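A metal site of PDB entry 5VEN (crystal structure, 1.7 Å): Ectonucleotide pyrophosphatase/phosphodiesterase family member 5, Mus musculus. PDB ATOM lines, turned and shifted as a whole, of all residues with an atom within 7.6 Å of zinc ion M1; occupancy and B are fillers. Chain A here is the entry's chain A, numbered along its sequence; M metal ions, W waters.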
ATOM      1  N   SER A  20      -1.543 -16.014 -18.043  1.00  0.00           N
ATOM      2  CA  SER A  20      -2.344 -17.196 -17.750  1.00  0.00           C
ATOM      3  C   SER A  20      -3.801 -16.888 -18.082  1.00  0.00           C
ATOM      4  O   SER A  20      -4.398 -15.980 -17.476  1.00  0.00           O
ATOM      5  CB  SER A  20      -2.208 -17.633 -16.310  1.00  0.00           C
ATOM      6  OG  SER A  20      -3.101 -18.705 -16.070  1.00  0.00           O
ATOM      7  N   PHE A  21      -4.343 -17.618 -19.060  1.00  0.00           N
ATOM      8  CA  PHE A  21      -5.786 -17.670 -19.292  1.00  0.00           C
ATOM      9  C   PHE A  21      -6.287 -18.875 -18.534  1.00  0.00           C
ATOM     10  O   PHE A  21      -5.968 -20.007 -18.901  1.00  0.00           O
ATOM     11  CB  PHE A  21      -6.097 -17.770 -20.784  1.00  0.00           C
ATOM     12  CG  PHE A  21      -5.729 -16.560 -21.574  1.00  0.00           C
ATOM     13  CD1 PHE A  21      -6.488 -15.380 -21.455  1.00  0.00           C
ATOM     14  CD2 PHE A  21      -4.650 -16.566 -22.438  1.00  0.00           C
ATOM     15  CE1 PHE A  21      -6.133 -14.260 -22.206  1.00  0.00           C
ATOM     16  CE2 PHE A  21      -4.336 -15.446 -23.179  1.00  0.00           C
ATOM     17  CZ  PHE A  21      -5.040 -14.308 -23.043  1.00  0.00           C
ATOM     18  N   ASP A  22      -7.025 -18.637 -17.438  1.00  0.00           N
ATOM     19  CA  ASP A  22      -7.419 -19.732 -16.543  1.00  0.00           C
ATOM     20  C   ASP A  22      -8.192 -20.796 -17.318  1.00  0.00           C
ATOM     21  O   ASP A  22      -9.083 -20.482 -18.106  1.00  0.00           O
ATOM     22  CB  ASP A  22      -8.255 -19.172 -15.393  1.00  0.00           C
ATOM     23  CG  ASP A  22      -8.221 -20.077 -14.186  1.00  0.00           C
ATOM     24  OD1 ASP A  22      -8.602 -21.255 -14.343  1.00  0.00           O
ATOM     25  OD2 ASP A  22      -7.782 -19.650 -13.103  1.00  0.00           O
ATOM     26  N   GLY A  23      -7.830 -22.056 -17.079  1.00  0.00           N
ATOM     27  CA  GLY A  23      -8.617 -23.167 -17.589  1.00  0.00           C
ATOM     28  C   GLY A  23      -8.538 -23.314 -19.091  1.00  0.00           C
ATOM     29  O   GLY A  23      -9.509 -23.770 -19.712  1.00  0.00           O
ATOM     30  N   PHE A  24      -7.403 -22.978 -19.698  1.00  0.00           N
ATOM     31  CA  PHE A  24      -7.248 -23.073 -21.158  1.00  0.00           C
ATOM     32  C   PHE A  24      -6.642 -24.427 -21.472  1.00  0.00           C
ATOM     33  O   PHE A  24      -5.404 -24.622 -21.442  1.00  0.00           O
ATOM     34  CB  PHE A  24      -6.422 -21.915 -21.711  1.00  0.00           C
ATOM     35  CG  PHE A  24      -6.617 -21.683 -23.180  1.00  0.00           C
ATOM     36  CD1 PHE A  24      -6.261 -22.651 -24.136  1.00  0.00           C
ATOM     37  CD2 PHE A  24      -7.199 -20.498 -23.622  1.00  0.00           C
ATOM     38  CE1 PHE A  24      -6.430 -22.399 -25.472  1.00  0.00           C
ATOM     39  CE2 PHE A  24      -7.378 -20.265 -24.987  1.00  0.00           C
ATOM     40  CZ  PHE A  24      -7.002 -21.237 -25.885  1.00  0.00           C
ATOM     41  N   THR A  56      -5.364 -30.514  -9.782  1.00  0.00           N
ATOM     42  CA  THR A  56      -5.282 -29.677 -10.981  1.00  0.00           C
ATOM     43  C   THR A  56      -6.283 -28.521 -10.851  1.00  0.00           C
ATOM     44  O   THR A  56      -7.230 -28.331 -11.657  1.00  0.00           O
ATOM     45  CB  THR A  56      -5.516 -30.531 -12.241  1.00  0.00           C
ATOM     46  OG1 THR A  56      -6.735 -31.262 -12.089  1.00  0.00           O
ATOM     47  CG2 THR A  56      -4.324 -31.449 -12.455  1.00  0.00           C
ATOM     48  N   LYS A  57      -6.069 -27.718  -9.794  1.00  0.00           N
ATOM     49  CA  LYS A  57      -6.854 -26.531  -9.448  1.00  0.00           C
ATOM     50  C   LYS A  57      -5.980 -25.273  -9.553  1.00  0.00           C
ATOM     51  O   LYS A  57      -4.758 -25.345  -9.715  1.00  0.00           O
ATOM     52  CB  LYS A  57      -7.437 -26.609  -8.019  1.00  0.00           C
ATOM     53  CG  LYS A  57      -8.439 -27.730  -7.746  1.00  0.00           C
ATOM     54  CD  LYS A  57      -9.787 -27.492  -8.314  1.00  0.00           C
ATOM     55  CE  LYS A  57     -10.752 -28.517  -7.756  1.00  0.00           C
ATOM     56  NZ  LYS A  57     -12.090 -28.145  -8.137  1.00  0.00           N
ATOM     57  N   THR A  58      -6.653 -24.125  -9.443  1.00  0.00           N
ATOM     58  CA  THR A  58      -6.072 -22.837  -9.814  1.00  0.00           C
ATOM     59  C   THR A  58      -4.927 -22.433  -8.877  1.00  0.00           C
ATOM     60  O   THR A  58      -3.837 -22.084  -9.338  1.00  0.00           O
ATOM     61  CB  THR A  58      -7.150 -21.762  -9.836  1.00  0.00           C
ATOM     62  OG1 THR A  58      -8.093 -22.064 -10.908  1.00  0.00           O
ATOM     63  CG2 THR A  58      -6.594 -20.388 -10.114  1.00  0.00           C
ATOM     64  N   TYR A  59      -5.175 -22.412  -7.572  1.00  0.00           N
ATOM     65  CA  TYR A  59      -4.137 -21.849  -6.691  1.00  0.00           C
ATOM     66  C   TYR A  59      -2.917 -22.761  -6.571  1.00  0.00           C
ATOM     67  O   TYR A  59      -1.785 -22.258  -6.704  1.00  0.00           O
ATOM     68  CB  TYR A  59      -4.745 -21.459  -5.345  1.00  0.00           C
ATOM     69  CG  TYR A  59      -5.276 -20.037  -5.439  1.00  0.00           C
ATOM     70  CD1 TYR A  59      -6.174 -19.668  -6.437  1.00  0.00           C
ATOM     71  CD2 TYR A  59      -4.785 -19.048  -4.645  1.00  0.00           C
ATOM     72  CE1 TYR A  59      -6.622 -18.332  -6.530  1.00  0.00           C
ATOM     73  CE2 TYR A  59      -5.224 -17.772  -4.732  1.00  0.00           C
ATOM     74  CZ  TYR A  59      -6.119 -17.398  -5.675  1.00  0.00           C
ATOM     75  OH  TYR A  59      -6.485 -16.061  -5.720  1.00  0.00           O
ATOM     76  N   ASN A  61      -1.742 -24.677  -8.909  1.00  0.00           N
ATOM     77  CA  ASN A  61      -0.978 -24.676 -10.140  1.00  0.00           C
ATOM     78  C   ASN A  61      -0.335 -23.341 -10.451  1.00  0.00           C
ATOM     79  O   ASN A  61       0.801 -23.326 -10.962  1.00  0.00           O
ATOM     80  CB  ASN A  61      -1.840 -25.176 -11.300  1.00  0.00           C
ATOM     81  CG  ASN A  61      -1.752 -26.682 -11.397  1.00  0.00           C
ATOM     82  OD1 ASN A  61      -0.783 -27.217 -11.930  1.00  0.00           O
ATOM     83  ND2 ASN A  61      -2.646 -27.365 -10.714  1.00  0.00           N
ATOM     84  N   HIS A  62      -0.980 -22.227 -10.099  1.00  0.00           N
ATOM     85  CA  HIS A  62      -0.308 -20.941 -10.291  1.00  0.00           C
ATOM     86  C   HIS A  62       0.885 -20.816  -9.348  1.00  0.00           C
ATOM     87  O   HIS A  62       1.937 -20.298  -9.743  1.00  0.00           O
ATOM     88  CB  HIS A  62      -1.256 -19.776 -10.142  1.00  0.00           C
ATOM     89  CG  HIS A  62      -2.113 -19.526 -11.353  1.00  0.00           C
ATOM     90  ND1 HIS A  62      -3.356 -20.094 -11.478  1.00  0.00           N
ATOM     91  CD2 HIS A  62      -1.910 -18.785 -12.480  1.00  0.00           C
ATOM     92  CE1 HIS A  62      -3.910 -19.702 -12.628  1.00  0.00           C
ATOM     93  NE2 HIS A  62      -3.049 -18.909 -13.248  1.00  0.00           N
ATOM     94  N   ASN A  79      -7.528 -25.142  -3.287  1.00  0.00           N
ATOM     95  CA  ASN A  79      -8.168 -23.835  -3.159  1.00  0.00           C
ATOM     96  C   ASN A  79      -8.862 -23.679  -1.816  1.00  0.00           C
ATOM     97  O   ASN A  79      -9.166 -22.557  -1.424  1.00  0.00           O
ATOM     98  CB  ASN A  79      -9.217 -23.609  -4.260  1.00  0.00           C
ATOM     99  CG  ASN A  79      -8.652 -23.572  -5.636  1.00  0.00           C
ATOM    100  OD1 ASN A  79      -7.466 -23.272  -5.866  1.00  0.00           O
ATOM    101  ND2 ASN A  79      -9.514 -23.849  -6.603  1.00  0.00           N
ATOM    102  N   LEU A  92     -10.611 -19.980  -1.398  1.00  0.00           N
ATOM    103  CA  LEU A  92     -10.764 -19.097  -2.556  1.00  0.00           C
ATOM    104  C   LEU A  92     -12.177 -18.539  -2.660  1.00  0.00           C
ATOM    105  O   LEU A  92     -12.363 -17.347  -2.956  1.00  0.00           O
ATOM    106  CB  LEU A  92     -10.404 -19.861  -3.825  1.00  0.00           C
ATOM    107  CG  LEU A  92     -10.513 -19.114  -5.130  1.00  0.00           C
ATOM    108  CD1 LEU A  92      -9.718 -17.790  -5.082  1.00  0.00           C
ATOM    109  CD2 LEU A  92     -10.008 -20.043  -6.229  1.00  0.00           C
ATOM    110  N   PRO A 126      -3.047 -15.017  -9.444  1.00  0.00           N
ATOM    111  CA  PRO A 126      -3.362 -15.629  -8.146  1.00  0.00           C
ATOM    112  C   PRO A 126      -2.197 -15.587  -7.168  1.00  0.00           C
ATOM    113  O   PRO A 126      -1.091 -16.069  -7.467  1.00  0.00           O
ATOM    114  CB  PRO A 126      -3.722 -17.084  -8.530  1.00  0.00           C
ATOM    115  CG  PRO A 126      -4.314 -16.928  -9.843  1.00  0.00           C
ATOM    116  CD  PRO A 126      -3.494 -15.866 -10.551  1.00  0.00           C
ATOM    117  N   TYR A 172      -3.219 -12.145 -15.787  1.00  0.00           N
ATOM    118  CA  TYR A 172      -4.153 -13.236 -15.548  1.00  0.00           C
ATOM    119  C   TYR A 172      -5.549 -12.827 -16.000  1.00  0.00           C
ATOM    120  O   TYR A 172      -5.951 -11.644 -15.860  1.00  0.00           O
ATOM    121  CB  TYR A 172      -4.147 -13.603 -14.074  1.00  0.00           C
ATOM    122  CG  TYR A 172      -5.222 -14.585 -13.640  1.00  0.00           C
ATOM    123  CD1 TYR A 172      -5.087 -15.966 -13.826  1.00  0.00           C
ATOM    124  CD2 TYR A 172      -6.345 -14.120 -12.973  1.00  0.00           C
ATOM    125  CE1 TYR A 172      -6.061 -16.840 -13.407  1.00  0.00           C
ATOM    126  CE2 TYR A 172      -7.307 -14.989 -12.504  1.00  0.00           C
ATOM    127  CZ  TYR A 172      -7.173 -16.342 -12.745  1.00  0.00           C
ATOM    128  OH  TYR A 172      -8.147 -17.179 -12.304  1.00  0.00           O
ATOM    129  N   TRP A 173      -6.282 -13.809 -16.536  1.00  0.00           N
ATOM    130  CA  TRP A 173      -7.659 -13.634 -16.989  1.00  0.00           C
ATOM    131  C   TRP A 173      -8.439 -14.908 -16.663  1.00  0.00           C
ATOM    132  O   TRP A 173      -7.900 -16.008 -16.737  1.00  0.00           O
ATOM    133  CB  TRP A 173      -7.663 -13.356 -18.487  1.00  0.00           C
ATOM    134  CG  TRP A 173      -8.998 -13.012 -19.060  1.00  0.00           C
ATOM    135  CD1 TRP A 173      -9.716 -13.713 -20.005  1.00  0.00           C
ATOM    136  CD2 TRP A 173      -9.813 -11.873 -18.710  1.00  0.00           C
ATOM    137  NE1 TRP A 173     -10.899 -13.074 -20.271  1.00  0.00           N
ATOM    138  CE2 TRP A 173     -10.986 -11.952 -19.495  1.00  0.00           C
ATOM    139  CE3 TRP A 173      -9.661 -10.804 -17.833  1.00  0.00           C
ATOM    140  CZ2 TRP A 173     -12.005 -10.980 -19.413  1.00  0.00           C
ATOM    141  CZ3 TRP A 173     -10.672  -9.848 -17.767  1.00  0.00           C
ATOM    142  CH2 TRP A 173     -11.820  -9.954 -18.542  1.00  0.00           C
ATOM    143  N   GLU A 174      -9.723 -14.744 -16.276  1.00  0.00           N
ATOM    144  CA  GLU A 174     -10.498 -15.822 -15.692  1.00  0.00           C
ATOM    145  C   GLU A 174     -11.175 -16.732 -16.716  1.00  0.00           C
ATOM    146  O   GLU A 174     -11.774 -17.729 -16.311  1.00  0.00           O
ATOM    147  CB  GLU A 174     -11.564 -15.230 -14.795  1.00  0.00           C
ATOM    148  CG  GLU A 174     -11.011 -14.519 -13.553  1.00  0.00           C
ATOM    149  CD  GLU A 174     -10.501 -13.077 -13.796  1.00  0.00           C
ATOM    150  OE1 GLU A 174      -9.834 -12.494 -12.905  1.00  0.00           O
ATOM    151  OE2 GLU A 174     -10.747 -12.505 -14.854  1.00  0.00           O
ATOM    152  N   ASP A 177     -11.891 -20.597 -18.260  1.00  0.00           N
ATOM    153  CA  ASP A 177     -12.295 -21.425 -17.122  1.00  0.00           C
ATOM    154  C   ASP A 177     -13.758 -21.194 -16.756  1.00  0.00           C
ATOM    155  O   ASP A 177     -14.512 -22.167 -16.574  1.00  0.00           O
ATOM    156  CB  ASP A 177     -11.411 -21.132 -15.919  1.00  0.00           C
ATOM    157  CG  ASP A 177     -11.851 -21.879 -14.671  1.00  0.00           C
ATOM    158  OD1 ASP A 177     -11.507 -23.057 -14.535  1.00  0.00           O
ATOM    159  OD2 ASP A 177     -12.582 -21.245 -13.842  1.00  0.00           O
ATOM    160  N   HIS A 181     -16.777 -24.105 -16.948  1.00  0.00           N
ATOM    161  CA  HIS A 181     -17.577 -24.645 -15.839  1.00  0.00           C
ATOM    162  C   HIS A 181     -19.067 -24.565 -16.135  1.00  0.00           C
ATOM    163  O   HIS A 181     -19.822 -25.539 -15.863  1.00  0.00           O
ATOM    164  CB  HIS A 181     -17.313 -23.847 -14.573  1.00  0.00           C
ATOM    165  CG  HIS A 181     -16.022 -24.160 -13.910  1.00  0.00           C
ATOM    166  ND1 HIS A 181     -15.764 -25.399 -13.360  1.00  0.00           N
ATOM    167  CD2 HIS A 181     -14.964 -23.378 -13.597  1.00  0.00           C
ATOM    168  CE1 HIS A 181     -14.559 -25.379 -12.795  1.00  0.00           C
ATOM    169  NE2 HIS A 181     -14.054 -24.168 -12.925  1.00  0.00           N
ATOM    170  N   SER A 223      -1.491 -21.690 -18.922  1.00  0.00           N
ATOM    171  CA  SER A 223      -2.667 -21.805 -18.089  1.00  0.00           C
ATOM    172  C   SER A 223      -2.311 -22.715 -16.934  1.00  0.00           C
ATOM    173  O   SER A 223      -1.207 -23.262 -16.885  1.00  0.00           O
ATOM    174  CB  SER A 223      -3.872 -22.297 -18.918  1.00  0.00           C
ATOM    175  OG  SER A 223      -5.057 -22.324 -18.146  1.00  0.00           O
ATOM    176  N   ASP A 224      -3.266 -22.882 -16.035  1.00  0.00           N
ATOM    177  CA  ASP A 224      -3.105 -23.676 -14.836  1.00  0.00           C
ATOM    178  C   ASP A 224      -3.617 -25.114 -14.962  1.00  0.00           C
ATOM    179  O   ASP A 224      -3.081 -26.015 -14.314  1.00  0.00           O
ATOM    180  CB  ASP A 224      -3.796 -22.983 -13.667  1.00  0.00           C
ATOM    181  CG  ASP A 224      -5.243 -22.559 -13.914  1.00  0.00           C
ATOM    182  OD1 ASP A 224      -5.732 -22.543 -15.078  1.00  0.00           O
ATOM    183  OD2 ASP A 224      -5.907 -22.214 -12.887  1.00  0.00           O
ATOM    184  N   HIS A 225      -4.597 -25.335 -15.835  1.00  0.00           N
ATOM    185  CA  HIS A 225      -5.233 -26.647 -15.953  1.00  0.00           C
ATOM    186  C   HIS A 225      -6.227 -26.547 -17.107  1.00  0.00           C
ATOM    187  O   HIS A 225      -6.507 -25.459 -17.647  1.00  0.00           O
ATOM    188  CB  HIS A 225      -5.991 -27.053 -14.685  1.00  0.00           C
ATOM    189  CG  HIS A 225      -6.963 -26.000 -14.257  1.00  0.00           C
ATOM    190  ND1 HIS A 225      -8.121 -25.725 -14.954  1.00  0.00           N
ATOM    191  CD2 HIS A 225      -6.867 -25.069 -13.273  1.00  0.00           C
ATOM    192  CE1 HIS A 225      -8.700 -24.650 -14.423  1.00  0.00           C
ATOM    193  NE2 HIS A 225      -7.941 -24.216 -13.412  1.00  0.00           N
ATOM    194  N   GLY A 226      -6.771 -27.706 -17.461  1.00  0.00           N
ATOM    195  CA  GLY A 226      -7.841 -27.826 -18.477  1.00  0.00           C
ATOM    196  C   GLY A 226      -9.202 -27.926 -17.842  1.00  0.00           C
ATOM    197  O   GLY A 226      -9.530 -27.254 -16.858  1.00  0.00           O
ATOM    198  N   MET A 227     -10.020 -28.811 -18.401  1.00  0.00           N
ATOM    199  CA  MET A 227     -11.430 -28.886 -18.054  1.00  0.00           C
ATOM    200  C   MET A 227     -11.973 -30.190 -18.646  1.00  0.00           C
ATOM    201  O   MET A 227     -11.580 -30.566 -19.748  1.00  0.00           O
ATOM    202  CB  MET A 227     -12.186 -27.672 -18.620  1.00  0.00           C
ATOM    203  CG  MET A 227     -13.614 -27.526 -18.093  1.00  0.00           C
ATOM    204  SD  MET A 227     -13.822 -26.946 -16.398  1.00  0.00           S
ATOM    205  CE  MET A 227     -13.081 -25.334 -16.521  1.00  0.00           C
ATOM    206  N   HIS A 325     -12.491 -29.495 -13.111  1.00  0.00           N
ATOM    207  CA  HIS A 325     -11.100 -29.903 -13.172  1.00  0.00           C
ATOM    208  C   HIS A 325     -10.659 -30.149 -11.728  1.00  0.00           C
ATOM    209  O   HIS A 325     -11.415 -29.949 -10.780  1.00  0.00           O
ATOM    210  CB  HIS A 325     -10.249 -28.836 -13.863  1.00  0.00           C
ATOM    211  CG  HIS A 325     -10.437 -27.498 -13.258  1.00  0.00           C
ATOM    212  ND1 HIS A 325      -9.646 -27.028 -12.230  1.00  0.00           N
ATOM    213  CD2 HIS A 325     -11.375 -26.532 -13.476  1.00  0.00           C
ATOM    214  CE1 HIS A 325     -10.059 -25.822 -11.870  1.00  0.00           C
ATOM    215  NE2 HIS A 325     -11.135 -25.506 -12.587  1.00  0.00           N
HETATM  216 ZN    ZN M   1      -7.859 -22.273 -12.803  1.00  0.00          ZN
HETATM  217 ZN    ZN M   2     -12.101 -23.708 -12.669  1.00  0.00          ZN
HETATM  218  O   HOH W   1     -10.309 -22.276 -12.049  1.00  0.00           O
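OD2 of Asp 22 sits at hydrogen-bond distance from OH of Tyr 172 (2.6 Å). N of Asp 177 lies within hydrogen-bond range of O of Asp 22 (2.8 Å). OG of Ser 223 sits at hydrogen-bond distance from O of His 225 (3.5 Å). OD1 of Asp 224 sits at hydrogen-bond distance from OG of Ser 223 (3.1 Å). A ring nitrogen (ND1) of His 62 sits at hydrogen-bond distance from the backbone carbonyl oxygen (O) of Thr 58, at 3.0 Å. OD1 of Asp 224 sits at hydrogen-bond distance from N of Gly 23 (2.9 Å). The backbone carbonyl oxygen of Trp 173 lies within hydrogen-bond range of the backbone NH of Asp 22, 2.9 Å away. ND1 of His 325 lies close to ND1 of His 225, at 3.4 Å.
Zinc ion M1 is bound by OG1 of Thr 58 (1.9 Å), OD2 of Asp 224 (2.0 Å), OD1 of Asp 22 (2.0 Å), NE2 of His 225 (2.0 Å) and water W1 (2.6 Å). Slightly farther from zinc ion M1 lies the side-chain carboxylate (OD2) of Asp 22 (2.6 Å).
Within 4 Å of zinc ion M1: Asp 22, Thr 58, Asp 224 and His 225. The nearest printed residue that does not touch zinc ion M1 is Asp 177 (4.1 Å).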
